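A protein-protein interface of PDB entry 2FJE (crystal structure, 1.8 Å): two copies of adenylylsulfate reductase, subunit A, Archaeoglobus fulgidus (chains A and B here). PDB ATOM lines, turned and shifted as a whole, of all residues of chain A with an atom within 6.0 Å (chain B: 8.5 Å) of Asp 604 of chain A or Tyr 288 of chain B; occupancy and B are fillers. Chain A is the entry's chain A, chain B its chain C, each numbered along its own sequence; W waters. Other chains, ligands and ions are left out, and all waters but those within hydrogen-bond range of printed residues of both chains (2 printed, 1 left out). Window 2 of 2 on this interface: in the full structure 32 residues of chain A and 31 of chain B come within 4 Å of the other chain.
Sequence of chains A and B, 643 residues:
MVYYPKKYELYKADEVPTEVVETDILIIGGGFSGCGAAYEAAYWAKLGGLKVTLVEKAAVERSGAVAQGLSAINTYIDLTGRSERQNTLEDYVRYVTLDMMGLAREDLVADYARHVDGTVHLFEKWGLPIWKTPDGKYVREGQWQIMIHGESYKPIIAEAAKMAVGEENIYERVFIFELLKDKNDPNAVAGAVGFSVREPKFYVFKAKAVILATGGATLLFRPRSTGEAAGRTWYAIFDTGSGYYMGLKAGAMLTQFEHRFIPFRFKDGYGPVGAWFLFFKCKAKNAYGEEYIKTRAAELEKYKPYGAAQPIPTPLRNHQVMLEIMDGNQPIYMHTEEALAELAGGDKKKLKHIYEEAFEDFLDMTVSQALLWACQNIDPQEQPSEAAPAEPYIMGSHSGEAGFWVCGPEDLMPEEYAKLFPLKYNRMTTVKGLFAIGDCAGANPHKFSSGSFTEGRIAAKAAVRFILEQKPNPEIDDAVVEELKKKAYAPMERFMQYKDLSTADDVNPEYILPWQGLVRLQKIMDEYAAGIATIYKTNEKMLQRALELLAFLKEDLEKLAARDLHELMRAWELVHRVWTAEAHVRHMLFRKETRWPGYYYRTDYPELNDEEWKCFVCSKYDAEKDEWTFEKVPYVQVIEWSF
OG1 of Thr 603 of chain A is in hydrogen-bond range of O of Gly 328 of chain B (3.1 Å). OD1 of Asn 539 of chain A lies close to O of Gly 328 of chain B (2.9 Å). The side-chain amide oxygen (OD1) of Asn 539 of chain A sits close to the backbone carbonyl oxygen (O) of Gln 330 of chain B (3.0 Å).
The backbone carbonyl oxygen (O) of Asn 329 of chain B lies within hydrogen-bond range of the backbone NH (N) of Ala 287 of chain B (2.9 Å). The side-chain amide nitrogen (ND2) of Asn 286 of chain B sits close to the backbone NH (N) of Tyr 288 of chain B, at 2.8 Å. The guanidinium group (NH2) of Arg 602 of chain A is in salt-bridge range of the side-chain carboxylate (OD2) of Asp 604 of chain A (2.8 Å). The side-chain amide nitrogen of Asn 539 of chain A lies close to the backbone NH of Lys 541 of chain A, at 3.0 Å. The backbone NH (N) of Glu 540 of chain A sits at hydrogen-bond distance from the side-chain carboxylate (OD2) of Asp 604 of chain A (3.0 Å). The backbone NH (N) of Thr 603 of chain A is in hydrogen-bond range of the backbone carbonyl oxygen (O) of Thr 538 of chain A (3.0 Å).
OD1 of Asn 539 of chain A touches OH of Tyr 288 of chain B, at 3.6 Å. CG of Lys 541 of chain A touches CB of Ala 287 of chain B (3.7 Å). Pro 331 of chain B touches Lys 541 of chain A. Thr 603 of chain A touches Asp 327 of chain B. CB of Asp 604 of chain A touches OH of Tyr 288 of chain B, at 3.5 Å.
Of chain B, only Tyr 288 comes within 4 Å of Asp 604 of chain A. Of chain A, only Asn 539 (3.6 Å) and Asp 604 (3.5 Å) come within 4 Å of Tyr 288 of chain B. Of the printed residues of chain B, Asn 539 of chain A touches Tyr 288 (3.6 Å), Gly 328 (2.9 Å) and Gln 330 (3.0 Å). Printed residues of chain B within 4 Å of Thr 603 of chain A: Asp 327 (3.7 Å) and Gly 328 (3.1 Å). Tyr 605 of chain A touches none of the printed residues of chain B. His 335 of chain B touches none of the printed residues of chain A. The nearest residue of chain B that does not touch Asp 604 of chain A is Gly 328 of chain B (6.1 Å). The nearest printed residue of chain A that does not touch Gln 330 of chain B is Lys 541 of chain A (4.4 Å).
Of the 17 printed residues of chain B, 6 touch a printed residue of chain A. Printed residues of chain A that touch a printed residue of chain B: Asn 539, Lys 541, Thr 603 and Asp 604. Among the printed residues, 8 pairs touch across the chains. Among the printed residues, no Asp or Glu carboxylate lies within 4 Å of a Lys or Arg side-chain nitrogen of the other chain.
No position is printed for both chains. Of the 8 pairs that touch across the chains among the printed residues, none has its exchanged pair printed and touching as well.
Water W1 lies within hydrogen-bond range of the side-chain hydroxyl of Thr 603 of chain A, the side-chain hydroxyl of Tyr 288 of chain B, the backbone carbonyl oxygen of Gly 328 of chain B and the side-chain amide oxygen of Asn 329 of chain B. Water W2 lies within hydrogen-bond range of the backbone carbonyl oxygen of Gly 328 of chain B (2.9 Å), the side-chain hydroxyl of Thr 603 of chain A (3.0 Å) and the backbone carbonyl oxygen of Thr 538 of chain A (3.3 Å).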
ATOM      1  N   THR A 538      14.125 -15.664  -8.665  1.00  0.00           N
ATOM      2  CA  THR A 538      13.652 -14.299  -8.492  1.00  0.00           C
ATOM      3  C   THR A 538      14.869 -13.384  -8.419  1.00  0.00           C
ATOM      4  O   THR A 538      16.010 -13.854  -8.447  1.00  0.00           O
ATOM      5  CB  THR A 538      12.780 -14.138  -7.211  1.00  0.00           C
ATOM      6  OG1 THR A 538      12.164 -12.842  -7.211  1.00  0.00           O
ATOM      7  CG2 THR A 538      13.624 -14.292  -5.949  1.00  0.00           C
ATOM      8  N   ASN A 539      14.625 -12.080  -8.370  1.00  0.00           N
ATOM      9  CA  ASN A 539      15.705 -11.105  -8.276  1.00  0.00           C
ATOM     10  C   ASN A 539      15.153  -9.825  -7.663  1.00  0.00           C
ATOM     11  O   ASN A 539      13.966  -9.756  -7.345  1.00  0.00           O
ATOM     12  CB  ASN A 539      16.346 -10.857  -9.660  1.00  0.00           C
ATOM     13  CG  ASN A 539      15.363 -10.329 -10.701  1.00  0.00           C
ATOM     14  OD1 ASN A 539      15.447 -10.681 -11.883  1.00  0.00           O
ATOM     15  ND2 ASN A 539      14.452  -9.473 -10.281  1.00  0.00           N
ATOM     16  N   GLU A 540      16.008  -8.825  -7.481  1.00  0.00           N
ATOM     17  CA  GLU A 540      15.593  -7.564  -6.876  1.00  0.00           C
ATOM     18  C   GLU A 540      14.384  -6.920  -7.551  1.00  0.00           C
ATOM     19  O   GLU A 540      13.419  -6.534  -6.885  1.00  0.00           O
ATOM     20  CB  GLU A 540      16.753  -6.570  -6.885  1.00  0.00           C
ATOM     21  CG  GLU A 540      16.436  -5.266  -6.182  1.00  0.00           C
ATOM     22  CD  GLU A 540      17.531  -4.232  -6.347  1.00  0.00           C
ATOM     23  OE1 GLU A 540      17.738  -3.763  -7.485  1.00  0.00           O
ATOM     24  OE2 GLU A 540      18.187  -3.896  -5.340  1.00  0.00           O
ATOM     25  N   LYS A 541      14.445  -6.800  -8.871  1.00  0.00           N
ATOM     26  CA  LYS A 541      13.364  -6.186  -9.636  1.00  0.00           C
ATOM     27  C   LYS A 541      12.032  -6.908  -9.473  1.00  0.00           C
ATOM     28  O   LYS A 541      10.997  -6.277  -9.261  1.00  0.00           O
ATOM     29  CB  LYS A 541      13.737  -6.147 -11.115  1.00  0.00           C
ATOM     30  CG  LYS A 541      15.059  -5.459 -11.398  1.00  0.00           C
ATOM     31  CD  LYS A 541      15.045  -4.012 -10.942  1.00  0.00           C
ATOM     32  CE  LYS A 541      16.352  -3.315 -11.302  1.00  0.00           C
ATOM     33  NZ  LYS A 541      16.411  -1.930 -10.747  1.00  0.00           N
ATOM     34  N   ARG A 602      18.380 -16.374  -6.116  1.00  0.00           N
ATOM     35  CA  ARG A 602      18.410 -14.936  -6.382  1.00  0.00           C
ATOM     36  C   ARG A 602      19.351 -14.908  -7.581  1.00  0.00           C
ATOM     37  O   ARG A 602      20.570 -14.993  -7.419  1.00  0.00           O
ATOM     38  CB  ARG A 602      19.045 -14.145  -5.229  1.00  0.00           C
ATOM     39  CG  ARG A 602      18.122 -13.775  -4.066  1.00  0.00           C
ATOM     40  CD  ARG A 602      17.112 -12.695  -4.438  1.00  0.00           C
ATOM     41  NE  ARG A 602      17.715 -11.436  -4.894  1.00  0.00           N
ATOM     42  CZ  ARG A 602      17.946 -10.369  -4.128  1.00  0.00           C
ATOM     43  NH1 ARG A 602      17.634 -10.378  -2.839  1.00  0.00           N
ATOM     44  NH2 ARG A 602      18.459  -9.269  -4.666  1.00  0.00           N
ATOM     45  N   THR A 603      18.798 -14.819  -8.784  1.00  0.00           N
ATOM     46  CA  THR A 603      19.638 -14.823  -9.974  1.00  0.00           C
ATOM     47  C   THR A 603      20.618 -13.655 -10.012  1.00  0.00           C
ATOM     48  O   THR A 603      21.627 -13.715 -10.715  1.00  0.00           O
ATOM     49  CB  THR A 603      18.785 -14.833 -11.254  1.00  0.00           C
ATOM     50  OG1 THR A 603      17.911 -13.700 -11.261  1.00  0.00           O
ATOM     51  CG2 THR A 603      17.947 -16.110 -11.315  1.00  0.00           C
ATOM     52  N   ASP A 604      20.334 -12.601  -9.250  1.00  0.00           N
ATOM     53  CA  ASP A 604      21.228 -11.449  -9.216  1.00  0.00           C
ATOM     54  C   ASP A 604      22.340 -11.604  -8.170  1.00  0.00           C
ATOM     55  O   ASP A 604      23.316 -10.856  -8.181  1.00  0.00           O
ATOM     56  CB  ASP A 604      20.434 -10.142  -9.013  1.00  0.00           C
ATOM     57  CG  ASP A 604      19.454 -10.198  -7.847  1.00  0.00           C
ATOM     58  OD1 ASP A 604      19.140 -11.298  -7.341  1.00  0.00           O
ATOM     59  OD2 ASP A 604      18.975  -9.114  -7.445  1.00  0.00           O
ATOM     60  N   TYR A 605      22.182 -12.581  -7.278  1.00  0.00           N
ATOM     61  CA  TYR A 605      23.170 -12.902  -6.241  1.00  0.00           C
ATOM     62  C   TYR A 605      23.122 -14.424  -6.119  1.00  0.00           C
ATOM     63  O   TYR A 605      22.737 -14.967  -5.085  1.00  0.00           O
ATOM     64  CB  TYR A 605      22.791 -12.265  -4.900  1.00  0.00           C
ATOM     65  CG  TYR A 605      22.805 -10.755  -4.905  1.00  0.00           C
ATOM     66  CD1 TYR A 605      21.634 -10.027  -5.106  1.00  0.00           C
ATOM     67  CD2 TYR A 605      23.995 -10.052  -4.714  1.00  0.00           C
ATOM     68  CE1 TYR A 605      21.645  -8.630  -5.113  1.00  0.00           C
ATOM     69  CE2 TYR A 605      24.019  -8.658  -4.721  1.00  0.00           C
ATOM     70  CZ  TYR A 605      22.843  -7.955  -4.919  1.00  0.00           C
ATOM     71  OH  TYR A 605      22.866  -6.580  -4.920  1.00  0.00           O
ATOM     72  N   PRO A 606      23.533 -15.129  -7.186  1.00  0.00           N
ATOM     73  CA  PRO A 606      23.558 -16.589  -7.313  1.00  0.00           C
ATOM     74  C   PRO A 606      24.432 -17.424  -6.388  1.00  0.00           C
ATOM     75  O   PRO A 606      24.273 -18.646  -6.335  1.00  0.00           O
ATOM     76  CB  PRO A 606      23.935 -16.788  -8.778  1.00  0.00           C
ATOM     77  CG  PRO A 606      24.891 -15.673  -9.005  1.00  0.00           C
ATOM     78  CD  PRO A 606      24.190 -14.501  -8.349  1.00  0.00           C
ATOM     79  N   LYS B 285      13.224  -4.508 -23.323  1.00  0.00           N
ATOM     80  CA  LYS B 285      14.446  -4.717 -22.553  1.00  0.00           C
ATOM     81  C   LYS B 285      14.186  -5.594 -21.340  1.00  0.00           C
ATOM     82  O   LYS B 285      13.050  -5.681 -20.870  1.00  0.00           O
ATOM     83  CB  LYS B 285      14.997  -3.370 -22.075  1.00  0.00           C
ATOM     84  CG  LYS B 285      15.314  -2.394 -23.200  1.00  0.00           C
ATOM     85  CD  LYS B 285      15.815  -1.070 -22.636  1.00  0.00           C
ATOM     86  CE  LYS B 285      16.105  -0.063 -23.743  1.00  0.00           C
ATOM     87  NZ  LYS B 285      16.640   1.214 -23.198  1.00  0.00           N
ATOM     88  N   ASN B 286      15.231  -6.241 -20.828  1.00  0.00           N
ATOM     89  CA  ASN B 286      15.058  -7.073 -19.641  1.00  0.00           C
ATOM     90  C   ASN B 286      15.110  -6.189 -18.396  1.00  0.00           C
ATOM     91  O   ASN B 286      15.173  -4.964 -18.505  1.00  0.00           O
ATOM     92  CB  ASN B 286      16.108  -8.199 -19.588  1.00  0.00           C
ATOM     93  CG  ASN B 286      17.532  -7.695 -19.398  1.00  0.00           C
ATOM     94  OD1 ASN B 286      18.487  -8.472 -19.497  1.00  0.00           O
ATOM     95  ND2 ASN B 286      17.684  -6.413 -19.112  1.00  0.00           N
ATOM     96  N   ALA B 287      15.079  -6.802 -17.219  1.00  0.00           N
ATOM     97  CA  ALA B 287      15.088  -6.055 -15.968  1.00  0.00           C
ATOM     98  C   ALA B 287      16.306  -5.156 -15.780  1.00  0.00           C
ATOM     99  O   ALA B 287      16.274  -4.225 -14.974  1.00  0.00           O
ATOM    100  CB  ALA B 287      14.974  -7.018 -14.791  1.00  0.00           C
ATOM    101  N   TYR B 288      17.375  -5.431 -16.519  1.00  0.00           N
ATOM    102  CA  TYR B 288      18.592  -4.639 -16.391  1.00  0.00           C
ATOM    103  C   TYR B 288      18.835  -3.692 -17.559  1.00  0.00           C
ATOM    104  O   TYR B 288      19.976  -3.320 -17.846  1.00  0.00           O
ATOM    105  CB  TYR B 288      19.785  -5.573 -16.197  1.00  0.00           C
ATOM    106  CG  TYR B 288      19.555  -6.565 -15.083  1.00  0.00           C
ATOM    107  CD1 TYR B 288      19.149  -7.872 -15.359  1.00  0.00           C
ATOM    108  CD2 TYR B 288      19.683  -6.183 -13.747  1.00  0.00           C
ATOM    109  CE1 TYR B 288      18.876  -8.773 -14.331  1.00  0.00           C
ATOM    110  CE2 TYR B 288      19.411  -7.074 -12.712  1.00  0.00           C
ATOM    111  CZ  TYR B 288      19.008  -8.366 -13.013  1.00  0.00           C
ATOM    112  OH  TYR B 288      18.733  -9.247 -11.995  1.00  0.00           O
ATOM    113  N   GLY B 289      17.754  -3.309 -18.230  1.00  0.00           N
ATOM    114  CA  GLY B 289      17.854  -2.382 -19.344  1.00  0.00           C
ATOM    115  C   GLY B 289      18.552  -2.881 -20.594  1.00  0.00           C
ATOM    116  O   GLY B 289      18.918  -2.083 -21.458  1.00  0.00           O
ATOM    117  N   GLU B 290      18.734  -4.190 -20.711  1.00  0.00           N
ATOM    118  CA  GLU B 290      19.394  -4.744 -21.886  1.00  0.00           C
ATOM    119  C   GLU B 290      18.409  -5.036 -23.007  1.00  0.00           C
ATOM    120  O   GLU B 290      17.391  -5.694 -22.792  1.00  0.00           O
ATOM    121  CB  GLU B 290      20.132  -6.033 -21.531  1.00  0.00           C
ATOM    122  CG  GLU B 290      21.260  -5.850 -20.536  1.00  0.00           C
ATOM    123  CD  GLU B 290      21.991  -7.147 -20.270  1.00  0.00           C
ATOM    124  OE1 GLU B 290      21.335  -8.118 -19.842  1.00  0.00           O
ATOM    125  OE2 GLU B 290      23.218  -7.193 -20.494  1.00  0.00           O
ATOM    126  N   GLU B 291      18.715  -4.538 -24.201  1.00  0.00           N
ATOM    127  CA  GLU B 291      17.872  -4.772 -25.368  1.00  0.00           C
ATOM    128  C   GLU B 291      18.306  -6.127 -25.918  1.00  0.00           C
ATOM    129  O   GLU B 291      19.222  -6.221 -26.738  1.00  0.00           O
ATOM    130  CB  GLU B 291      18.089  -3.658 -26.396  1.00  0.00           C
ATOM    131  CG  GLU B 291      17.351  -3.857 -27.703  1.00  0.00           C
ATOM    132  CD  GLU B 291      17.107  -2.552 -28.435  1.00  0.00           C
ATOM    133  OE1 GLU B 291      17.896  -1.600 -28.232  1.00  0.00           O
ATOM    134  OE2 GLU B 291      16.132  -2.485 -29.218  1.00  0.00           O
ATOM    135  N   THR B 295      21.556  -8.116 -27.566  1.00  0.00           N
ATOM    136  CA  THR B 295      22.447  -8.888 -26.708  1.00  0.00           C
ATOM    137  C   THR B 295      22.349 -10.393 -26.955  1.00  0.00           C
ATOM    138  O   THR B 295      23.266 -11.140 -26.620  1.00  0.00           O
ATOM    139  CB  THR B 295      22.169  -8.611 -25.212  1.00  0.00           C
ATOM    140  OG1 THR B 295      20.828  -8.997 -24.889  1.00  0.00           O
ATOM    141  CG2 THR B 295      22.357  -7.133 -24.903  1.00  0.00           C
ATOM    142  N   GLU B 324      16.212 -15.017 -21.874  1.00  0.00           N
ATOM    143  CA  GLU B 324      16.208 -14.016 -20.812  1.00  0.00           C
ATOM    144  C   GLU B 324      15.402 -14.527 -19.625  1.00  0.00           C
ATOM    145  O   GLU B 324      15.803 -14.368 -18.471  1.00  0.00           O
ATOM    146  CB  GLU B 324      15.593 -12.708 -21.309  1.00  0.00           C
ATOM    147  CG  GLU B 324      16.469 -11.935 -22.270  1.00  0.00           C
ATOM    148  CD  GLU B 324      17.809 -11.589 -21.658  1.00  0.00           C
ATOM    149  OE1 GLU B 324      17.834 -11.188 -20.476  1.00  0.00           O
ATOM    150  OE2 GLU B 324      18.831 -11.709 -22.360  1.00  0.00           O
ATOM    151  N   ASP B 327      17.216 -17.201 -17.784  1.00  0.00           N
ATOM    152  CA  ASP B 327      18.318 -16.648 -17.006  1.00  0.00           C
ATOM    153  C   ASP B 327      17.772 -15.895 -15.799  1.00  0.00           C
ATOM    154  O   ASP B 327      18.522 -15.513 -14.900  1.00  0.00           O
ATOM    155  CB  ASP B 327      19.173 -15.708 -17.863  1.00  0.00           C
ATOM    156  CG  ASP B 327      20.107 -16.459 -18.795  1.00  0.00           C
ATOM    157  OD1 ASP B 327      20.132 -17.706 -18.742  1.00  0.00           O
ATOM    158  OD2 ASP B 327      20.822 -15.803 -19.576  1.00  0.00           O
ATOM    159  N   GLY B 328      16.456 -15.699 -15.784  1.00  0.00           N
ATOM    160  CA  GLY B 328      15.814 -14.997 -14.688  1.00  0.00           C
ATOM    161  C   GLY B 328      16.014 -13.495 -14.764  1.00  0.00           C
ATOM    162  O   GLY B 328      16.172 -12.832 -13.737  1.00  0.00           O
ATOM    163  N   ASN B 329      16.001 -12.950 -15.977  1.00  0.00           N
ATOM    164  CA  ASN B 329      16.197 -11.516 -16.158  1.00  0.00           C
ATOM    165  C   ASN B 329      14.902 -10.733 -16.312  1.00  0.00           C
ATOM    166  O   ASN B 329      14.882  -9.666 -16.915  1.00  0.00           O
ATOM    167  CB  ASN B 329      17.106 -11.241 -17.358  1.00  0.00           C
ATOM    168  CG  ASN B 329      18.515 -11.755 -17.147  1.00  0.00           C
ATOM    169  OD1 ASN B 329      18.974 -11.887 -16.011  1.00  0.00           O
ATOM    170  ND2 ASN B 329      19.217 -12.034 -18.240  1.00  0.00           N
ATOM    171  N   GLN B 330      13.822 -11.271 -15.761  1.00  0.00           N
ATOM    172  CA  GLN B 330      12.535 -10.595 -15.806  1.00  0.00           C
ATOM    173  C   GLN B 330      12.524  -9.576 -14.671  1.00  0.00           C
ATOM    174  O   GLN B 330      13.334  -9.663 -13.750  1.00  0.00           O
ATOM    175  CB  GLN B 330      11.402 -11.602 -15.621  1.00  0.00           C
ATOM    176  CG  GLN B 330      11.203 -12.505 -16.815  1.00  0.00           C
ATOM    177  CD  GLN B 330       9.974 -13.375 -16.690  1.00  0.00           C
ATOM    178  OE1 GLN B 330       9.974 -14.373 -15.966  1.00  0.00           O
ATOM    179  NE2 GLN B 330       8.909 -12.996 -17.386  1.00  0.00           N
ATOM    180  N   PRO B 331      11.605  -8.601 -14.719  1.00  0.00           N
ATOM    181  CA  PRO B 331      10.591  -8.404 -15.761  1.00  0.00           C
ATOM    182  C   PRO B 331      11.150  -7.935 -17.098  1.00  0.00           C
ATOM    183  O   PRO B 331      12.201  -7.292 -17.160  1.00  0.00           O
ATOM    184  CB  PRO B 331       9.667  -7.340 -15.156  1.00  0.00           C
ATOM    185  CG  PRO B 331       9.914  -7.431 -13.682  1.00  0.00           C
ATOM    186  CD  PRO B 331      11.399  -7.646 -13.618  1.00  0.00           C
ATOM    187  N   ILE B 332      10.435  -8.276 -18.167  1.00  0.00           N
ATOM    188  CA  ILE B 332      10.785  -7.848 -19.518  1.00  0.00           C
ATOM    189  C   ILE B 332       9.867  -6.652 -19.743  1.00  0.00           C
ATOM    190  O   ILE B 332       8.654  -6.748 -19.536  1.00  0.00           O
ATOM    191  CB  ILE B 332      10.465  -8.932 -20.577  1.00  0.00           C
ATOM    192  CG1 ILE B 332      11.531 -10.037 -20.567  1.00  0.00           C
ATOM    193  CG2 ILE B 332      10.455  -8.299 -21.963  1.00  0.00           C
ATOM    194  CD1 ILE B 332      12.071 -10.402 -19.209  1.00  0.00           C
ATOM    195  N   TYR B 333      10.437  -5.526 -20.158  1.00  0.00           N
ATOM    196  CA  TYR B 333       9.644  -4.318 -20.360  1.00  0.00           C
ATOM    197  C   TYR B 333       9.535  -3.787 -21.777  1.00  0.00           C
ATOM    198  O   TYR B 333      10.481  -3.861 -22.559  1.00  0.00           O
ATOM    199  CB  TYR B 333      10.198  -3.168 -19.513  1.00  0.00           C
ATOM    200  CG  TYR B 333      10.054  -3.326 -18.024  1.00  0.00           C
ATOM    201  CD1 TYR B 333      11.115  -3.787 -17.246  1.00  0.00           C
ATOM    202  CD2 TYR B 333       8.863  -2.993 -17.386  1.00  0.00           C
ATOM    203  CE1 TYR B 333      10.994  -3.903 -15.870  1.00  0.00           C
ATOM    204  CE2 TYR B 333       8.731  -3.108 -16.009  1.00  0.00           C
ATOM    205  CZ  TYR B 333       9.800  -3.562 -15.258  1.00  0.00           C
ATOM    206  OH  TYR B 333       9.674  -3.673 -13.895  1.00  0.00           O
ATOM    207  N   HIS B 335       9.304  -0.454 -23.348  1.00  0.00           N
ATOM    208  CA  HIS B 335       9.526   0.926 -22.934  1.00  0.00           C
ATOM    209  C   HIS B 335       8.741   1.969 -23.720  1.00  0.00           C
ATOM    210  O   HIS B 335       9.294   2.775 -24.471  1.00  0.00           O
ATOM    211  CB  HIS B 335      11.027   1.215 -22.943  1.00  0.00           C
ATOM    212  CG  HIS B 335      11.740   0.639 -21.761  1.00  0.00           C
ATOM    213  ND1 HIS B 335      11.768   1.268 -20.535  1.00  0.00           N
ATOM    214  CD2 HIS B 335      12.366  -0.550 -21.586  1.00  0.00           C
ATOM    215  CE1 HIS B 335      12.376   0.491 -19.656  1.00  0.00           C
ATOM    216  NE2 HIS B 335      12.749  -0.618 -20.269  1.00  0.00           N
HETATM  217  O   HOH W   1      18.766 -11.885 -12.853  1.00  0.00           O
HETATM  218  O   HOH W   2      14.947 -14.208 -11.556  1.00  0.00           O
